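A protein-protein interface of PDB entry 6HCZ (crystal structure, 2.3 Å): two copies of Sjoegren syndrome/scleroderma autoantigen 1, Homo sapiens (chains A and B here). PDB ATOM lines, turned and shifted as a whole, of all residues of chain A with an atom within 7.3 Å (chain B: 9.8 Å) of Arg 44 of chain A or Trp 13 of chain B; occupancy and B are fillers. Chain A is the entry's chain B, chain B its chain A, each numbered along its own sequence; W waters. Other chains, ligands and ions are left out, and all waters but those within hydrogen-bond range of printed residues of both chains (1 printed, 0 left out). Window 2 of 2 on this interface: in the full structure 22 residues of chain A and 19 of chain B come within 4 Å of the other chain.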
ATOM      1  N   LEU A  37      19.488  -5.741 -34.954  1.00  0.00           N
ATOM      2  CA  LEU A  37      20.546  -4.907 -34.324  1.00  0.00           C
ATOM      3  C   LEU A  37      20.600  -5.040 -32.787  1.00  0.00           C
ATOM      4  O   LEU A  37      21.667  -5.059 -32.187  1.00  0.00           O
ATOM      5  CB  LEU A  37      20.276  -3.456 -34.693  1.00  0.00           C
ATOM      6  CG  LEU A  37      20.947  -3.000 -35.973  1.00  0.00           C
ATOM      7  CD1 LEU A  37      20.445  -1.615 -36.368  1.00  0.00           C
ATOM      8  CD2 LEU A  37      22.456  -3.021 -35.782  1.00  0.00           C
ATOM      9  N   MET A  38      19.438  -5.043 -32.136  1.00  0.00           N
ATOM     10  CA  MET A  38      19.376  -5.189 -30.728  1.00  0.00           C
ATOM     11  C   MET A  38      20.024  -6.529 -30.349  1.00  0.00           C
ATOM     12  O   MET A  38      20.836  -6.625 -29.422  1.00  0.00           O
ATOM     13  CB  MET A  38      17.912  -5.151 -30.260  1.00  0.00           C
ATOM     14  CG  MET A  38      17.739  -4.911 -28.754  1.00  0.00           C
ATOM     15  SD  MET A  38      15.989  -4.765 -28.339  1.00  0.00           S
ATOM     16  CE  MET A  38      15.608  -3.262 -29.243  1.00  0.00           C
ATOM     17  N   GLY A  39      19.622  -7.592 -31.054  1.00  0.00           N
ATOM     18  CA  GLY A  39      20.230  -8.909 -30.863  1.00  0.00           C
ATOM     19  C   GLY A  39      21.747  -8.869 -31.053  1.00  0.00           C
ATOM     20  O   GLY A  39      22.485  -9.403 -30.241  1.00  0.00           O
ATOM     21  N   ASP A  40      22.212  -8.207 -32.118  1.00  0.00           N
ATOM     22  CA  ASP A  40      23.632  -8.136 -32.419  1.00  0.00           C
ATOM     23  C   ASP A  40      24.391  -7.517 -31.251  1.00  0.00           C
ATOM     24  O   ASP A  40      25.362  -8.049 -30.805  1.00  0.00           O
ATOM     25  CB  ASP A  40      23.909  -7.365 -33.713  1.00  0.00           C
ATOM     26  CG  ASP A  40      25.346  -7.493 -34.209  1.00  0.00           C
ATOM     27  OD1 ASP A  40      25.868  -8.604 -34.184  1.00  0.00           O
ATOM     28  OD2 ASP A  40      25.930  -6.480 -34.606  1.00  0.00           O
ATOM     29  N   TYR A  41      23.906  -6.397 -30.742  1.00  0.00           N
ATOM     30  CA  TYR A  41      24.585  -5.692 -29.679  1.00  0.00           C
ATOM     31  C   TYR A  41      24.498  -6.448 -28.356  1.00  0.00           C
ATOM     32  O   TYR A  41      25.397  -6.362 -27.561  1.00  0.00           O
ATOM     33  CB  TYR A  41      23.989  -4.302 -29.499  1.00  0.00           C
ATOM     34  CG  TYR A  41      24.493  -3.273 -30.479  1.00  0.00           C
ATOM     35  CD1 TYR A  41      25.796  -2.789 -30.401  1.00  0.00           C
ATOM     36  CD2 TYR A  41      23.664  -2.755 -31.460  1.00  0.00           C
ATOM     37  CE1 TYR A  41      26.253  -1.827 -31.280  1.00  0.00           C
ATOM     38  CE2 TYR A  41      24.103  -1.783 -32.342  1.00  0.00           C
ATOM     39  CZ  TYR A  41      25.399  -1.309 -32.243  1.00  0.00           C
ATOM     40  OH  TYR A  41      25.817  -0.334 -33.101  1.00  0.00           O
ATOM     41  N   LEU A  42      23.382  -7.126 -28.098  1.00  0.00           N
ATOM     42  CA  LEU A  42      23.296  -8.010 -26.929  1.00  0.00           C
ATOM     43  C   LEU A  42      24.369  -9.105 -27.044  1.00  0.00           C
ATOM     44  O   LEU A  42      24.998  -9.486 -26.043  1.00  0.00           O
ATOM     45  CB  LEU A  42      21.923  -8.678 -26.876  1.00  0.00           C
ATOM     46  CG  LEU A  42      20.785  -7.809 -26.384  1.00  0.00           C
ATOM     47  CD1 LEU A  42      19.465  -8.523 -26.610  1.00  0.00           C
ATOM     48  CD2 LEU A  42      20.965  -7.456 -24.920  1.00  0.00           C
ATOM     49  N   LEU A  43      24.525  -9.653 -28.260  1.00  0.00           N
ATOM     50  CA  LEU A  43      25.505 -10.722 -28.490  1.00  0.00           C
ATOM     51  C   LEU A  43      26.909 -10.136 -28.313  1.00  0.00           C
ATOM     52  O   LEU A  43      27.709 -10.778 -27.648  1.00  0.00           O
ATOM     53  CB  LEU A  43      25.291 -11.357 -29.861  1.00  0.00           C
ATOM     54  CG  LEU A  43      24.052 -12.236 -29.973  1.00  0.00           C
ATOM     55  CD1 LEU A  43      23.736 -12.557 -31.426  1.00  0.00           C
ATOM     56  CD2 LEU A  43      24.208 -13.495 -29.138  1.00  0.00           C
ATOM     57  N   ARG A  44      27.122  -8.884 -28.752  1.00  0.00           N
ATOM     58  CA  ARG A  44      28.406  -8.170 -28.602  1.00  0.00           C
ATOM     59  C   ARG A  44      28.604  -7.681 -27.166  1.00  0.00           C
ATOM     60  O   ARG A  44      29.577  -7.009 -26.885  1.00  0.00           O
ATOM     61  CB  ARG A  44      28.516  -7.000 -29.594  1.00  0.00           C
ATOM     62  CG  ARG A  44      28.459  -7.446 -31.066  1.00  0.00           C
ATOM     63  CD  ARG A  44      28.056  -6.345 -32.040  1.00  0.00           C
ATOM     64  NE  ARG A  44      29.261  -5.602 -32.402  1.00  0.00           N
ATOM     65  CZ  ARG A  44      29.324  -4.289 -32.616  1.00  0.00           C
ATOM     66  NH1 ARG A  44      28.233  -3.538 -32.501  1.00  0.00           N
ATOM     67  NH2 ARG A  44      30.485  -3.734 -32.956  1.00  0.00           N
ATOM     68  N   GLY A  45      27.672  -7.974 -26.255  1.00  0.00           N
ATOM     69  CA  GLY A  45      27.923  -7.726 -24.816  1.00  0.00           C
ATOM     70  C   GLY A  45      27.190  -6.533 -24.196  1.00  0.00           C
ATOM     71  O   GLY A  45      27.378  -6.280 -23.010  1.00  0.00           O
ATOM     72  N   TYR A  46      26.350  -5.807 -24.958  1.00  0.00           N
ATOM     73  CA  TYR A  46      25.565  -4.621 -24.437  1.00  0.00           C
ATOM     74  C   TYR A  46      24.538  -5.132 -23.397  1.00  0.00           C
ATOM     75  O   TYR A  46      24.126  -6.252 -23.444  1.00  0.00           O
ATOM     76  CB  TYR A  46      24.862  -3.885 -25.615  1.00  0.00           C
ATOM     77  CG  TYR A  46      25.712  -2.977 -26.495  1.00  0.00           C
ATOM     78  CD1 TYR A  46      27.057  -3.137 -26.727  1.00  0.00           C
ATOM     79  CD2 TYR A  46      25.101  -1.900 -27.127  1.00  0.00           C
ATOM     80  CE1 TYR A  46      27.777  -2.240 -27.532  1.00  0.00           C
ATOM     81  CE2 TYR A  46      25.817  -1.034 -27.943  1.00  0.00           C
ATOM     82  CZ  TYR A  46      27.161  -1.199 -28.155  1.00  0.00           C
ATOM     83  OH  TYR A  46      27.825  -0.343 -28.981  1.00  0.00           O
ATOM     84  N   ASP A  63      26.015   0.223 -23.036  1.00  0.00           N
ATOM     85  CA  ASP A  63      27.335  -0.234 -23.362  1.00  0.00           C
ATOM     86  C   ASP A  63      28.218   0.075 -22.144  1.00  0.00           C
ATOM     87  O   ASP A  63      28.583   1.243 -21.935  1.00  0.00           O
ATOM     88  CB  ASP A  63      27.783   0.447 -24.696  1.00  0.00           C
ATOM     89  CG  ASP A  63      29.269   0.320 -25.006  1.00  0.00           C
ATOM     90  OD1 ASP A  63      29.854  -0.757 -24.663  1.00  0.00           O
ATOM     91  OD2 ASP A  63      29.835   1.320 -25.570  1.00  0.00           O
ATOM     92  N   LYS A  64      28.522  -0.968 -21.342  1.00  0.00           N
ATOM     93  CA  LYS A  64      29.316  -0.867 -20.089  1.00  0.00           C
ATOM     94  C   LYS A  64      28.804   0.319 -19.243  1.00  0.00           C
ATOM     95  O   LYS A  64      27.616   0.394 -18.963  1.00  0.00           O
ATOM     96  CB  LYS A  64      30.812  -0.781 -20.420  1.00  0.00           C
ATOM     97  CG  LYS A  64      31.379  -2.003 -21.132  1.00  0.00           C
ATOM     98  CD  LYS A  64      32.731  -1.782 -21.793  1.00  0.00           C
ATOM     99  CE  LYS A  64      33.220  -3.006 -22.547  1.00  0.00           C
ATOM    100  NZ  LYS A  64      34.699  -3.008 -22.666  1.00  0.00           N
ATOM    101  N   GLU A  75      20.991   4.645 -35.078  1.00  0.00           N
ATOM    102  CA  GLU A  75      21.653   3.879 -36.185  1.00  0.00           C
ATOM    103  C   GLU A  75      20.768   3.748 -37.443  1.00  0.00           C
ATOM    104  O   GLU A  75      21.215   4.031 -38.543  1.00  0.00           O
ATOM    105  CB  GLU A  75      22.130   2.501 -35.692  1.00  0.00           C
ATOM    106  CG  GLU A  75      23.303   1.919 -36.507  1.00  0.00           C
ATOM    107  CD  GLU A  75      24.149   0.852 -35.814  1.00  0.00           C
ATOM    108  OE1 GLU A  75      24.257   0.899 -34.571  1.00  0.00           O
ATOM    109  OE2 GLU A  75      24.720  -0.030 -36.526  1.00  0.00           O
ATOM    110  N   SER B  12      36.997  -9.317 -20.998  1.00  0.00           N
ATOM    111  CA  SER B  12      35.644  -9.844 -20.676  1.00  0.00           C
ATOM    112  C   SER B  12      34.553  -8.948 -21.295  1.00  0.00           C
ATOM    113  O   SER B  12      34.738  -7.740 -21.509  1.00  0.00           O
ATOM    114  CB  SER B  12      35.470 -10.005 -19.186  1.00  0.00           C
ATOM    115  OG  SER B  12      35.280  -8.744 -18.575  1.00  0.00           O
ATOM    116  N   TRP B  13      33.391  -9.572 -21.513  1.00  0.00           N
ATOM    117  CA  TRP B  13      32.417  -9.179 -22.497  1.00  0.00           C
ATOM    118  C   TRP B  13      31.045  -9.700 -22.048  1.00  0.00           C
ATOM    119  O   TRP B  13      30.034  -8.974 -22.141  1.00  0.00           O
ATOM    120  CB  TRP B  13      32.837  -9.700 -23.888  1.00  0.00           C
ATOM    121  CG  TRP B  13      31.798 -10.494 -24.626  1.00  0.00           C
ATOM    122  CD1 TRP B  13      30.928 -10.011 -25.559  1.00  0.00           C
ATOM    123  CD2 TRP B  13      31.510 -11.904 -24.518  1.00  0.00           C
ATOM    124  NE1 TRP B  13      30.120 -11.011 -26.031  1.00  0.00           N
ATOM    125  CE2 TRP B  13      30.442 -12.180 -25.402  1.00  0.00           C
ATOM    126  CE3 TRP B  13      32.040 -12.962 -23.766  1.00  0.00           C
ATOM    127  CZ2 TRP B  13      29.895 -13.456 -25.550  1.00  0.00           C
ATOM    128  CZ3 TRP B  13      31.507 -14.225 -23.913  1.00  0.00           C
ATOM    129  CH2 TRP B  13      30.442 -14.465 -24.788  1.00  0.00           C
ATOM    130  N   GLU B  14      31.017 -10.948 -21.553  1.00  0.00           N
ATOM    131  CA  GLU B  14      29.845 -11.536 -20.885  1.00  0.00           C
ATOM    132  C   GLU B  14      28.738 -11.837 -21.897  1.00  0.00           C
ATOM    133  O   GLU B  14      28.401 -11.006 -22.740  1.00  0.00           O
ATOM    134  CB  GLU B  14      29.337 -10.617 -19.768  1.00  0.00           C
ATOM    135  CG  GLU B  14      30.311 -10.494 -18.596  1.00  0.00           C
ATOM    136  CD  GLU B  14      30.559  -9.081 -18.079  1.00  0.00           C
ATOM    137  OE1 GLU B  14      29.581  -8.306 -17.974  1.00  0.00           O
ATOM    138  OE2 GLU B  14      31.735  -8.756 -17.790  1.00  0.00           O
ATOM    139  N   PRO B  15      28.118 -13.037 -21.843  1.00  0.00           N
ATOM    140  CA  PRO B  15      26.959 -13.333 -22.674  1.00  0.00           C
ATOM    141  C   PRO B  15      25.754 -12.450 -22.370  1.00  0.00           C
ATOM    142  O   PRO B  15      25.713 -11.751 -21.364  1.00  0.00           O
ATOM    143  CB  PRO B  15      26.590 -14.792 -22.364  1.00  0.00           C
ATOM    144  CG  PRO B  15      27.811 -15.358 -21.669  1.00  0.00           C
ATOM    145  CD  PRO B  15      28.506 -14.182 -21.010  1.00  0.00           C
ATOM    146  N   PRO B  16      24.765 -12.403 -23.287  1.00  0.00           N
ATOM    147  CA  PRO B  16      23.413 -11.968 -22.945  1.00  0.00           C
ATOM    148  C   PRO B  16      22.777 -12.925 -21.934  1.00  0.00           C
ATOM    149  O   PRO B  16      23.057 -14.105 -21.972  1.00  0.00           O
ATOM    150  CB  PRO B  16      22.654 -12.066 -24.275  1.00  0.00           C
ATOM    151  CG  PRO B  16      23.464 -13.049 -25.095  1.00  0.00           C
ATOM    152  CD  PRO B  16      24.895 -12.756 -24.710  1.00  0.00           C
ATOM    153  N   THR B  17      21.926 -12.395 -21.053  1.00  0.00           N
ATOM    154  CA  THR B  17      21.319 -13.190 -20.018  1.00  0.00           C
ATOM    155  C   THR B  17      20.056 -13.854 -20.549  1.00  0.00           C
ATOM    156  O   THR B  17      19.579 -13.530 -21.653  1.00  0.00           O
ATOM    157  CB  THR B  17      20.962 -12.341 -18.800  1.00  0.00           C
ATOM    158  OG1 THR B  17      19.861 -11.544 -19.226  1.00  0.00           O
ATOM    159  CG2 THR B  17      22.112 -11.486 -18.320  1.00  0.00           C
ATOM    160  N   GLU B  20      17.367 -11.190 -20.963  1.00  0.00           N
ATOM    161  CA  GLU B  20      17.553 -10.384 -22.149  1.00  0.00           C
ATOM    162  C   GLU B  20      16.994 -11.113 -23.372  1.00  0.00           C
ATOM    163  O   GLU B  20      16.189 -10.570 -24.111  1.00  0.00           O
ATOM    164  CB  GLU B  20      19.028 -10.034 -22.305  1.00  0.00           C
ATOM    165  CG  GLU B  20      19.473  -8.995 -21.298  1.00  0.00           C
ATOM    166  CD  GLU B  20      20.970  -8.817 -21.138  1.00  0.00           C
ATOM    167  OE1 GLU B  20      21.697  -9.846 -21.062  1.00  0.00           O
ATOM    168  OE2 GLU B  20      21.403  -7.647 -21.072  1.00  0.00           O
HETATM  169  O   HOH W   1      24.213  -8.544 -22.317  1.00  0.00           O
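O of Leu 43 of chain A lies within hydrogen-bond range of NE1 of Trp 13 of chain B, at 2.9 Å.
The backbone carbonyl oxygen of Tyr 41 of chain A is in hydrogen-bond range of the backbone NH of Tyr 46 of chain A (2.8 Å).
The backbone NH (N) of Thr 17 of chain B sits at hydrogen-bond distance from the side-chain carboxylate (OE1) of Glu 20 of chain B.
Among the printed residues, merely in contact across the chains: Leu 42 of chain A with Pro 16 of chain B (3.5 Å), Arg 44 of chain A with Trp 13 of chain B (3.5 Å), Gly 45 of chain A with Trp 13 of chain B (3.6 Å), Tyr 46 of chain A with Glu 20 of chain B (3.9 Å), Leu 42 of chain A with Glu 20 of chain B (3.9 Å) and Gly 45 of chain A with Glu 14 of chain B (3.9 Å).
Leu 43 of chain A touches just one residue of chain B: Trp 13.
Of the printed residues of chain B, Gly 45 of chain A touches Trp 13 and Glu 14.
Of the printed residues of chain B, Tyr 46 of chain A touches Glu 20.
Trp 13 of chain B touches three residues of chain A.
Of the printed residues of chain A, Pro 16 of chain B touches Leu 42 (3.5 Å).
The nearest residue of chain A that does not touch Trp 13 of chain B is Leu 42 of chain A (5.3 Å).
Of the 7 printed residues of chain B, 4 touch a printed residue of chain A.
Hydrophobic or aromatic side chains of chain B that line the printed part of chain A: Trp 13 and Pro 16.
Printed residues of chain A that touch a printed residue of chain B: Leu 42, Leu 43, Arg 44, Gly 45 and Tyr 46.
Hydrophobic or aromatic side chains of chain A within 4 Å of the printed part of chain B: Leu 42.
Along chain A the printed residues that touch a printed residue of chain B span positions 42 to 46.
Among the printed residues, no Asp or Glu carboxylate lies within 4 Å of a Lys or Arg side-chain nitrogen of the other chain.
No position is printed for both chains.
Water W1 lies within hydrogen-bond range of O of Tyr 46 of chain A (2.6 Å) and OE1 of Glu 20 of chain B (3.1 Å).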
